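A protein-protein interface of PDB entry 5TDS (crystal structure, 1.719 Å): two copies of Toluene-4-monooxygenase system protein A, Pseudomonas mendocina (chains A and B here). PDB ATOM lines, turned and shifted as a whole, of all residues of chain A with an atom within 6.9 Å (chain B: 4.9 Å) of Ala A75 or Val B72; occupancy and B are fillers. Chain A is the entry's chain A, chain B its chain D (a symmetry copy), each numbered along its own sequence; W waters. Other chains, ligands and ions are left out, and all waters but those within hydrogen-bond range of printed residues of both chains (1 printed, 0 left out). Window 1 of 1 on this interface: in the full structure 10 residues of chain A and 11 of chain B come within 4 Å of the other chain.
OG of Ser B71 lies within hydrogen-bond range of O of Gly B68 (3.0 Å).
CA of Gly A68 touches OG of Ser B71, at 3.5 Å.
OG of Ser A71 touches CA of Gly B68 (3.4 Å).
OG of Ser B71 touches CB of Ser A71, at 3.6 Å.
Val B72 touches Ser A71 (CG2 to O, 3.6 Å).
Ser B71 touches Val A72 (O to CG2, 3.8 Å).
Val A72 touches Ala B75.
Ala A75 touches Val B72 (CB to CG2, 3.6 Å).
Ala A75 touches Tyr B218.
O of Arg A78 touches OH of Tyr B218 (3.7 Å).
Ala A79 touches Tyr B218 (CA to OH, 3.7 Å).
Of chain B, only Val B72 (3.6 Å), Tyr B218 (3.7 Å) and Asn B222 (3.97 Å) come within 4 Å of Ala A75.
Of the printed residues of chain A, Val B72 touches Ser A71 (3.6 Å) and Ala A75 (3.6 Å).
Of the printed residues of chain A, Ala B75 touches Val A72.
Of the printed residues of chain A, Gly B68 touches Ser A71.
Printed residues of chain A within 4 Å of Tyr B218: Ala A75, Leu A76, Arg A78 and Ala A79.
Of the printed residues of chain B, Leu A76 touches Leu B76 (3.9 Å) and Tyr B218 (3.4 Å).
Of the printed residues of chain B, Val A72 touches Ser B71 and Ala B75.
Tyr A70 touches none of the printed residues of chain B.
The nearest residue of chain A that does not touch Val B72 is Val A72 (4.02 Å).
The nearest printed residue of chain B that does not touch Leu A76 is Val B72 (6.1 Å).
Hydrophobic or aromatic side chains of chain A within 4 Å of the printed part of chain B: Val A72, Ala A75 and Leu A76.
Among the printed residues, 13 pairs touch across the chains.
Among the printed residues, no Asp or Glu carboxylate lies within 4 Å of a Lys or Arg side-chain nitrogen of the other chain.
Gly A68 touches Ser B71, and with the chains exchanged Ser A71 touches Gly B68.
Ser A71 touches Val B72, and with the chains exchanged Val A72 touches Ser B71.
Val A72 touches Ala B75, and with the chains exchanged Ala A75 touches Val B72.
Leu A76 touches its own counterpart, Leu B76.
Positions printed for both chains: 68, 70, 71, 72, 73, 74, 75, 76 and 219.
Of the 13 pairs that touch across the chains among the printed residues, 8 have their exchanged pair printed and touching as well.
Water W1 bridges O of Ala A75 and O of Tyr B218.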
ATOM      1  N   GLY A  68      11.020  30.678 -16.973  1.00  0.00           N
ATOM      2  CA  GLY A  68       9.953  29.804 -17.417  1.00  0.00           C
ATOM      3  C   GLY A  68      10.069  28.387 -16.878  1.00  0.00           C
ATOM      4  O   GLY A  68       9.095  27.833 -16.364  1.00  0.00           O
ATOM      5  N   TYR A  70      11.544  27.018 -14.264  1.00  0.00           N
ATOM      6  CA  TYR A  70      11.307  26.826 -12.833  1.00  0.00           C
ATOM      7  C   TYR A  70       9.896  27.254 -12.417  1.00  0.00           C
ATOM      8  O   TYR A  70       9.317  26.665 -11.511  1.00  0.00           O
ATOM      9  CB  TYR A  70      12.361  27.570 -12.005  1.00  0.00           C
ATOM     10  CG  TYR A  70      13.745  26.938 -12.092  1.00  0.00           C
ATOM     11  CD1 TYR A  70      14.626  27.286 -13.106  1.00  0.00           C
ATOM     12  CD2 TYR A  70      14.164  25.983 -11.170  1.00  0.00           C
ATOM     13  CE1 TYR A  70      15.889  26.706 -13.200  1.00  0.00           C
ATOM     14  CE2 TYR A  70      15.438  25.394 -11.257  1.00  0.00           C
ATOM     15  CZ  TYR A  70      16.291  25.765 -12.276  1.00  0.00           C
ATOM     16  OH  TYR A  70      17.553  25.193 -12.390  1.00  0.00           O
ATOM     17  N   SER A  71       9.338  28.264 -13.074  1.00  0.00           N
ATOM     18  CA  SER A  71       7.971  28.682 -12.757  1.00  0.00           C
ATOM     19  C   SER A  71       6.969  27.590 -13.099  1.00  0.00           C
ATOM     20  O   SER A  71       5.996  27.379 -12.372  1.00  0.00           O
ATOM     21  CB  SER A  71       7.607  29.968 -13.497  1.00  0.00           C
ATOM     22  OG  SER A  71       8.387  31.048 -13.019  1.00  0.00           O
ATOM     23  N   VAL A  72       7.208  26.889 -14.200  1.00  0.00           N
ATOM     24  CA  VAL A  72       6.292  25.832 -14.617  1.00  0.00           C
ATOM     25  C   VAL A  72       6.384  24.645 -13.666  1.00  0.00           C
ATOM     26  O   VAL A  72       5.364  24.099 -13.244  1.00  0.00           O
ATOM     27  CB  VAL A  72       6.570  25.393 -16.065  1.00  0.00           C
ATOM     28  CG1 VAL A  72       5.764  24.152 -16.424  1.00  0.00           C
ATOM     29  CG2 VAL A  72       6.247  26.540 -17.020  1.00  0.00           C
ATOM     30  N   LYS A  73       7.608  24.242 -13.326  1.00  0.00           N
ATOM     31  CA  LYS A  73       7.805  23.211 -12.313  1.00  0.00           C
ATOM     32  C   LYS A  73       7.029  23.526 -11.029  1.00  0.00           C
ATOM     33  O   LYS A  73       6.321  22.671 -10.496  1.00  0.00           O
ATOM     34  CB  LYS A  73       9.296  23.054 -11.996  1.00  0.00           C
ATOM     35  CG  LYS A  73       9.606  21.926 -11.028  1.00  0.00           C
ATOM     36  CD  LYS A  73      11.097  21.913 -10.683  1.00  0.00           C
ATOM     37  CE  LYS A  73      11.442  20.822  -9.657  1.00  0.00           C
ATOM     38  NZ  LYS A  73      10.664  20.968  -8.394  1.00  0.00           N
ATOM     39  N   ALA A  74       7.135  24.762 -10.551  1.00  0.00           N
ATOM     40  CA  ALA A  74       6.468  25.136  -9.306  1.00  0.00           C
ATOM     41  C   ALA A  74       4.945  25.117  -9.450  1.00  0.00           C
ATOM     42  O   ALA A  74       4.235  24.661  -8.554  1.00  0.00           O
ATOM     43  CB  ALA A  74       6.935  26.507  -8.850  1.00  0.00           C
ATOM     44  N   ALA A  75       4.446  25.612 -10.578  1.00  0.00           N
ATOM     45  CA  ALA A  75       3.004  25.749 -10.768  1.00  0.00           C
ATOM     46  C   ALA A  75       2.310  24.395 -10.949  1.00  0.00           C
ATOM     47  O   ALA A  75       1.101  24.284 -10.743  1.00  0.00           O
ATOM     48  CB  ALA A  75       2.718  26.656 -11.965  1.00  0.00           C
ATOM     49  N   LEU A  76       3.072  23.371 -11.335  1.00  0.00           N
ATOM     50  CA  LEU A  76       2.500  22.048 -11.606  1.00  0.00           C
ATOM     51  C   LEU A  76       2.832  21.016 -10.530  1.00  0.00           C
ATOM     52  O   LEU A  76       2.609  19.817 -10.722  1.00  0.00           O
ATOM     53  CB  LEU A  76       2.978  21.528 -12.965  1.00  0.00           C
ATOM     54  CG  LEU A  76       2.326  22.160 -14.195  1.00  0.00           C
ATOM     55  CD1 LEU A  76       2.942  21.619 -15.471  1.00  0.00           C
ATOM     56  CD2 LEU A  76       0.828  21.911 -14.182  1.00  0.00           C
ATOM     57  N   GLU A  77       3.357  21.461  -9.397  1.00  0.00           N
ATOM     58  CA  GLU A  77       3.800  20.495  -8.396  1.00  0.00           C
ATOM     59  C   GLU A  77       2.621  19.717  -7.795  1.00  0.00           C
ATOM     60  O   GLU A  77       2.819  18.653  -7.213  1.00  0.00           O
ATOM     61  CB  GLU A  77       4.635  21.185  -7.303  1.00  0.00           C
ATOM     62  CG  GLU A  77       6.109  21.378  -7.736  1.00  0.00           C
ATOM     63  CD  GLU A  77       7.029  21.942  -6.652  1.00  0.00           C
ATOM     64  OE1 GLU A  77       7.936  21.208  -6.200  1.00  0.00           O
ATOM     65  OE2 GLU A  77       6.874  23.126  -6.273  1.00  0.00           O
ATOM     66  N   ARG A  78       1.400  20.216  -7.967  1.00  0.00           N
ATOM     67  CA  ARG A  78       0.214  19.491  -7.495  1.00  0.00           C
ATOM     68  C   ARG A  78      -0.272  18.444  -8.501  1.00  0.00           C
ATOM     69  O   ARG A  78      -1.180  17.663  -8.201  1.00  0.00           O
ATOM     70  CB  ARG A  78      -0.939  20.453  -7.198  1.00  0.00           C
ATOM     71  CG  ARG A  78      -0.802  21.297  -5.943  1.00  0.00           C
ATOM     72  CD  ARG A  78      -2.138  21.978  -5.663  1.00  0.00           C
ATOM     73  NE  ARG A  78      -2.039  23.139  -4.780  1.00  0.00           N
ATOM     74  CZ  ARG A  78      -2.148  24.403  -5.185  1.00  0.00           C
ATOM     75  NH1 ARG A  78      -2.351  24.683  -6.468  1.00  0.00           N
ATOM     76  NH2 ARG A  78      -2.050  25.393  -4.306  1.00  0.00           N
ATOM     77  N   ALA A  79       0.313  18.431  -9.692  1.00  0.00           N
ATOM     78  CA  ALA A  79      -0.134  17.514 -10.739  1.00  0.00           C
ATOM     79  C   ALA A  79       0.122  16.047 -10.389  1.00  0.00           C
ATOM     80  O   ALA A  79      -0.506  15.157 -10.955  1.00  0.00           O
ATOM     81  CB  ALA A  79       0.530  17.855 -12.059  1.00  0.00           C
ATOM     82  N   THR A 219       5.720  19.594 -17.219  1.00  0.00           N
ATOM     83  CA  THR A 219       6.940  20.109 -16.594  1.00  0.00           C
ATOM     84  C   THR A 219       8.170  19.580 -17.322  1.00  0.00           C
ATOM     85  O   THR A 219       9.082  20.330 -17.653  1.00  0.00           O
ATOM     86  CB  THR A 219       7.034  19.728 -15.107  1.00  0.00           C
ATOM     87  OG1 THR A 219       6.002  20.402 -14.384  1.00  0.00           O
ATOM     88  CG2 THR A 219       8.385  20.127 -14.539  1.00  0.00           C
ATOM     89  N   GLY B  68       6.640  34.611 -14.343  1.00  0.00           N
ATOM     90  CA  GLY B  68       6.069  33.334 -13.965  1.00  0.00           C
ATOM     91  C   GLY B  68       4.690  33.095 -14.555  1.00  0.00           C
ATOM     92  O   GLY B  68       4.429  32.035 -15.131  1.00  0.00           O
ATOM     93  N   ALA B  69       3.797  34.073 -14.411  1.00  0.00           N
ATOM     94  CA  ALA B  69       2.400  33.873 -14.809  1.00  0.00           C
ATOM     95  C   ALA B  69       2.280  33.568 -16.295  1.00  0.00           C
ATOM     96  O   ALA B  69       1.569  32.645 -16.694  1.00  0.00           O
ATOM     97  CB  ALA B  69       1.552  35.098 -14.452  1.00  0.00           C
ATOM     98  N   TYR B  70       2.978  34.338 -17.116  1.00  0.00           N
ATOM     99  CA  TYR B  70       2.863  34.162 -18.559  1.00  0.00           C
ATOM    100  C   TYR B  70       3.591  32.910 -19.042  1.00  0.00           C
ATOM    101  O   TYR B  70       3.153  32.268 -19.988  1.00  0.00           O
ATOM    102  CB  TYR B  70       3.382  35.394 -19.295  1.00  0.00           C
ATOM    103  CG  TYR B  70       2.461  36.598 -19.196  1.00  0.00           C
ATOM    104  CD1 TYR B  70       2.547  37.486 -18.128  1.00  0.00           C
ATOM    105  CD2 TYR B  70       1.507  36.849 -20.173  1.00  0.00           C
ATOM    106  CE1 TYR B  70       1.707  38.597 -18.038  1.00  0.00           C
ATOM    107  CE2 TYR B  70       0.668  37.951 -20.090  1.00  0.00           C
ATOM    108  CZ  TYR B  70       0.772  38.819 -19.022  1.00  0.00           C
ATOM    109  OH  TYR B  70      -0.074  39.907 -18.946  1.00  0.00           O
ATOM    110  N   SER B  71       4.691  32.548 -18.393  1.00  0.00           N
ATOM    111  CA  SER B  71       5.415  31.363 -18.837  1.00  0.00           C
ATOM    112  C   SER B  71       4.607  30.094 -18.520  1.00  0.00           C
ATOM    113  O   SER B  71       4.615  29.125 -19.289  1.00  0.00           O
ATOM    114  CB  SER B  71       6.817  31.315 -18.212  1.00  0.00           C
ATOM    115  OG  SER B  71       6.760  31.172 -16.812  1.00  0.00           O
ATOM    116  N   VAL B  72       3.889  30.099 -17.402  1.00  0.00           N
ATOM    117  CA  VAL B  72       3.036  28.963 -17.065  1.00  0.00           C
ATOM    118  C   VAL B  72       1.911  28.824 -18.090  1.00  0.00           C
ATOM    119  O   VAL B  72       1.658  27.733 -18.584  1.00  0.00           O
ATOM    120  CB  VAL B  72       2.458  29.095 -15.630  1.00  0.00           C
ATOM    121  CG1 VAL B  72       1.378  28.065 -15.377  1.00  0.00           C
ATOM    122  CG2 VAL B  72       3.575  28.947 -14.603  1.00  0.00           C
ATOM    123  N   LYS B  73       1.252  29.928 -18.431  1.00  0.00           N
ATOM    124  CA  LYS B  73       0.200  29.884 -19.444  1.00  0.00           C
ATOM    125  C   LYS B  73       0.716  29.270 -20.744  1.00  0.00           C
ATOM    126  O   LYS B  73       0.078  28.391 -21.327  1.00  0.00           O
ATOM    127  CB  LYS B  73      -0.353  31.288 -19.705  1.00  0.00           C
ATOM    128  CG  LYS B  73      -1.425  31.357 -20.805  1.00  0.00           C
ATOM    129  CD  LYS B  73      -1.766  32.808 -21.124  1.00  0.00           C
ATOM    130  CE  LYS B  73      -2.931  32.930 -22.097  1.00  0.00           C
ATOM    131  NZ  LYS B  73      -2.646  32.314 -23.426  1.00  0.00           N
ATOM    132  N   ALA B  74       1.877  29.727 -21.195  1.00  0.00           N
ATOM    133  CA  ALA B  74       2.419  29.279 -22.474  1.00  0.00           C
ATOM    134  C   ALA B  74       2.744  27.791 -22.461  1.00  0.00           C
ATOM    135  O   ALA B  74       2.506  27.084 -23.451  1.00  0.00           O
ATOM    136  CB  ALA B  74       3.666  30.090 -22.836  1.00  0.00           C
ATOM    137  N   ALA B  75       3.277  27.306 -21.342  1.00  0.00           N
ATOM    138  CA  ALA B  75       3.721  25.917 -21.276  1.00  0.00           C
ATOM    139  C   ALA B  75       2.551  24.938 -21.188  1.00  0.00           C
ATOM    140  O   ALA B  75       2.711  23.743 -21.449  1.00  0.00           O
ATOM    141  CB  ALA B  75       4.666  25.724 -20.085  1.00  0.00           C
ATOM    142  N   LEU B  76       1.380  25.434 -20.804  1.00  0.00           N
ATOM    143  CA  LEU B  76       0.209  24.571 -20.666  1.00  0.00           C
ATOM    144  C   LEU B  76      -0.774  24.753 -21.816  1.00  0.00           C
ATOM    145  O   LEU B  76      -1.890  24.236 -21.772  1.00  0.00           O
ATOM    146  CB  LEU B  76      -0.483  24.829 -19.331  1.00  0.00           C
ATOM    147  CG  LEU B  76       0.289  24.278 -18.128  1.00  0.00           C
ATOM    148  CD1 LEU B  76      -0.445  24.548 -16.822  1.00  0.00           C
ATOM    149  CD2 LEU B  76       0.544  22.788 -18.307  1.00  0.00           C
ATOM    150  N   TYR B 218      -4.239  24.542 -13.603  1.00  0.00           N
ATOM    151  CA  TYR B 218      -3.091  25.116 -12.908  1.00  0.00           C
ATOM    152  C   TYR B 218      -2.676  26.484 -13.454  1.00  0.00           C
ATOM    153  O   TYR B 218      -2.084  27.280 -12.731  1.00  0.00           O
ATOM    154  CB  TYR B 218      -1.919  24.133 -12.951  1.00  0.00           C
ATOM    155  CG  TYR B 218      -2.299  22.810 -12.338  1.00  0.00           C
ATOM    156  CD1 TYR B 218      -2.591  22.715 -10.984  1.00  0.00           C
ATOM    157  CD2 TYR B 218      -2.401  21.666 -13.115  1.00  0.00           C
ATOM    158  CE1 TYR B 218      -2.962  21.507 -10.417  1.00  0.00           C
ATOM    159  CE2 TYR B 218      -2.772  20.458 -12.559  1.00  0.00           C
ATOM    160  CZ  TYR B 218      -3.052  20.384 -11.211  1.00  0.00           C
ATOM    161  OH  TYR B 218      -3.423  19.178 -10.660  1.00  0.00           O
ATOM    162  N   THR B 219      -3.000  26.769 -14.714  1.00  0.00           N
ATOM    163  CA  THR B 219      -2.757  28.100 -15.254  1.00  0.00           C
ATOM    164  C   THR B 219      -3.583  29.141 -14.512  1.00  0.00           C
ATOM    165  O   THR B 219      -3.067  30.185 -14.104  1.00  0.00           O
ATOM    166  CB  THR B 219      -3.092  28.180 -16.746  1.00  0.00           C
ATOM    167  OG1 THR B 219      -2.183  27.352 -17.477  1.00  0.00           O
ATOM    168  CG2 THR B 219      -2.980  29.619 -17.234  1.00  0.00           C
ATOM    169  N   ASN B 222      -2.551  29.491 -10.809  1.00  0.00           N
ATOM    170  CA  ASN B 222      -1.345  30.298 -10.712  1.00  0.00           C
ATOM    171  C   ASN B 222      -1.654  31.787 -10.928  1.00  0.00           C
ATOM    172  O   ASN B 222      -1.155  32.650 -10.210  1.00  0.00           O
ATOM    173  CB  ASN B 222      -0.314  29.805 -11.721  1.00  0.00           C
ATOM    174  CG  ASN B 222       1.059  30.397 -11.485  1.00  0.00           C
ATOM    175  OD1 ASN B 222       1.675  30.171 -10.441  1.00  0.00           O
ATOM    176  ND2 ASN B 222       1.553  31.141 -12.461  1.00  0.00           N
HETATM  177  O   HOH W   1      -0.703  26.218 -10.246  1.00  0.00           O
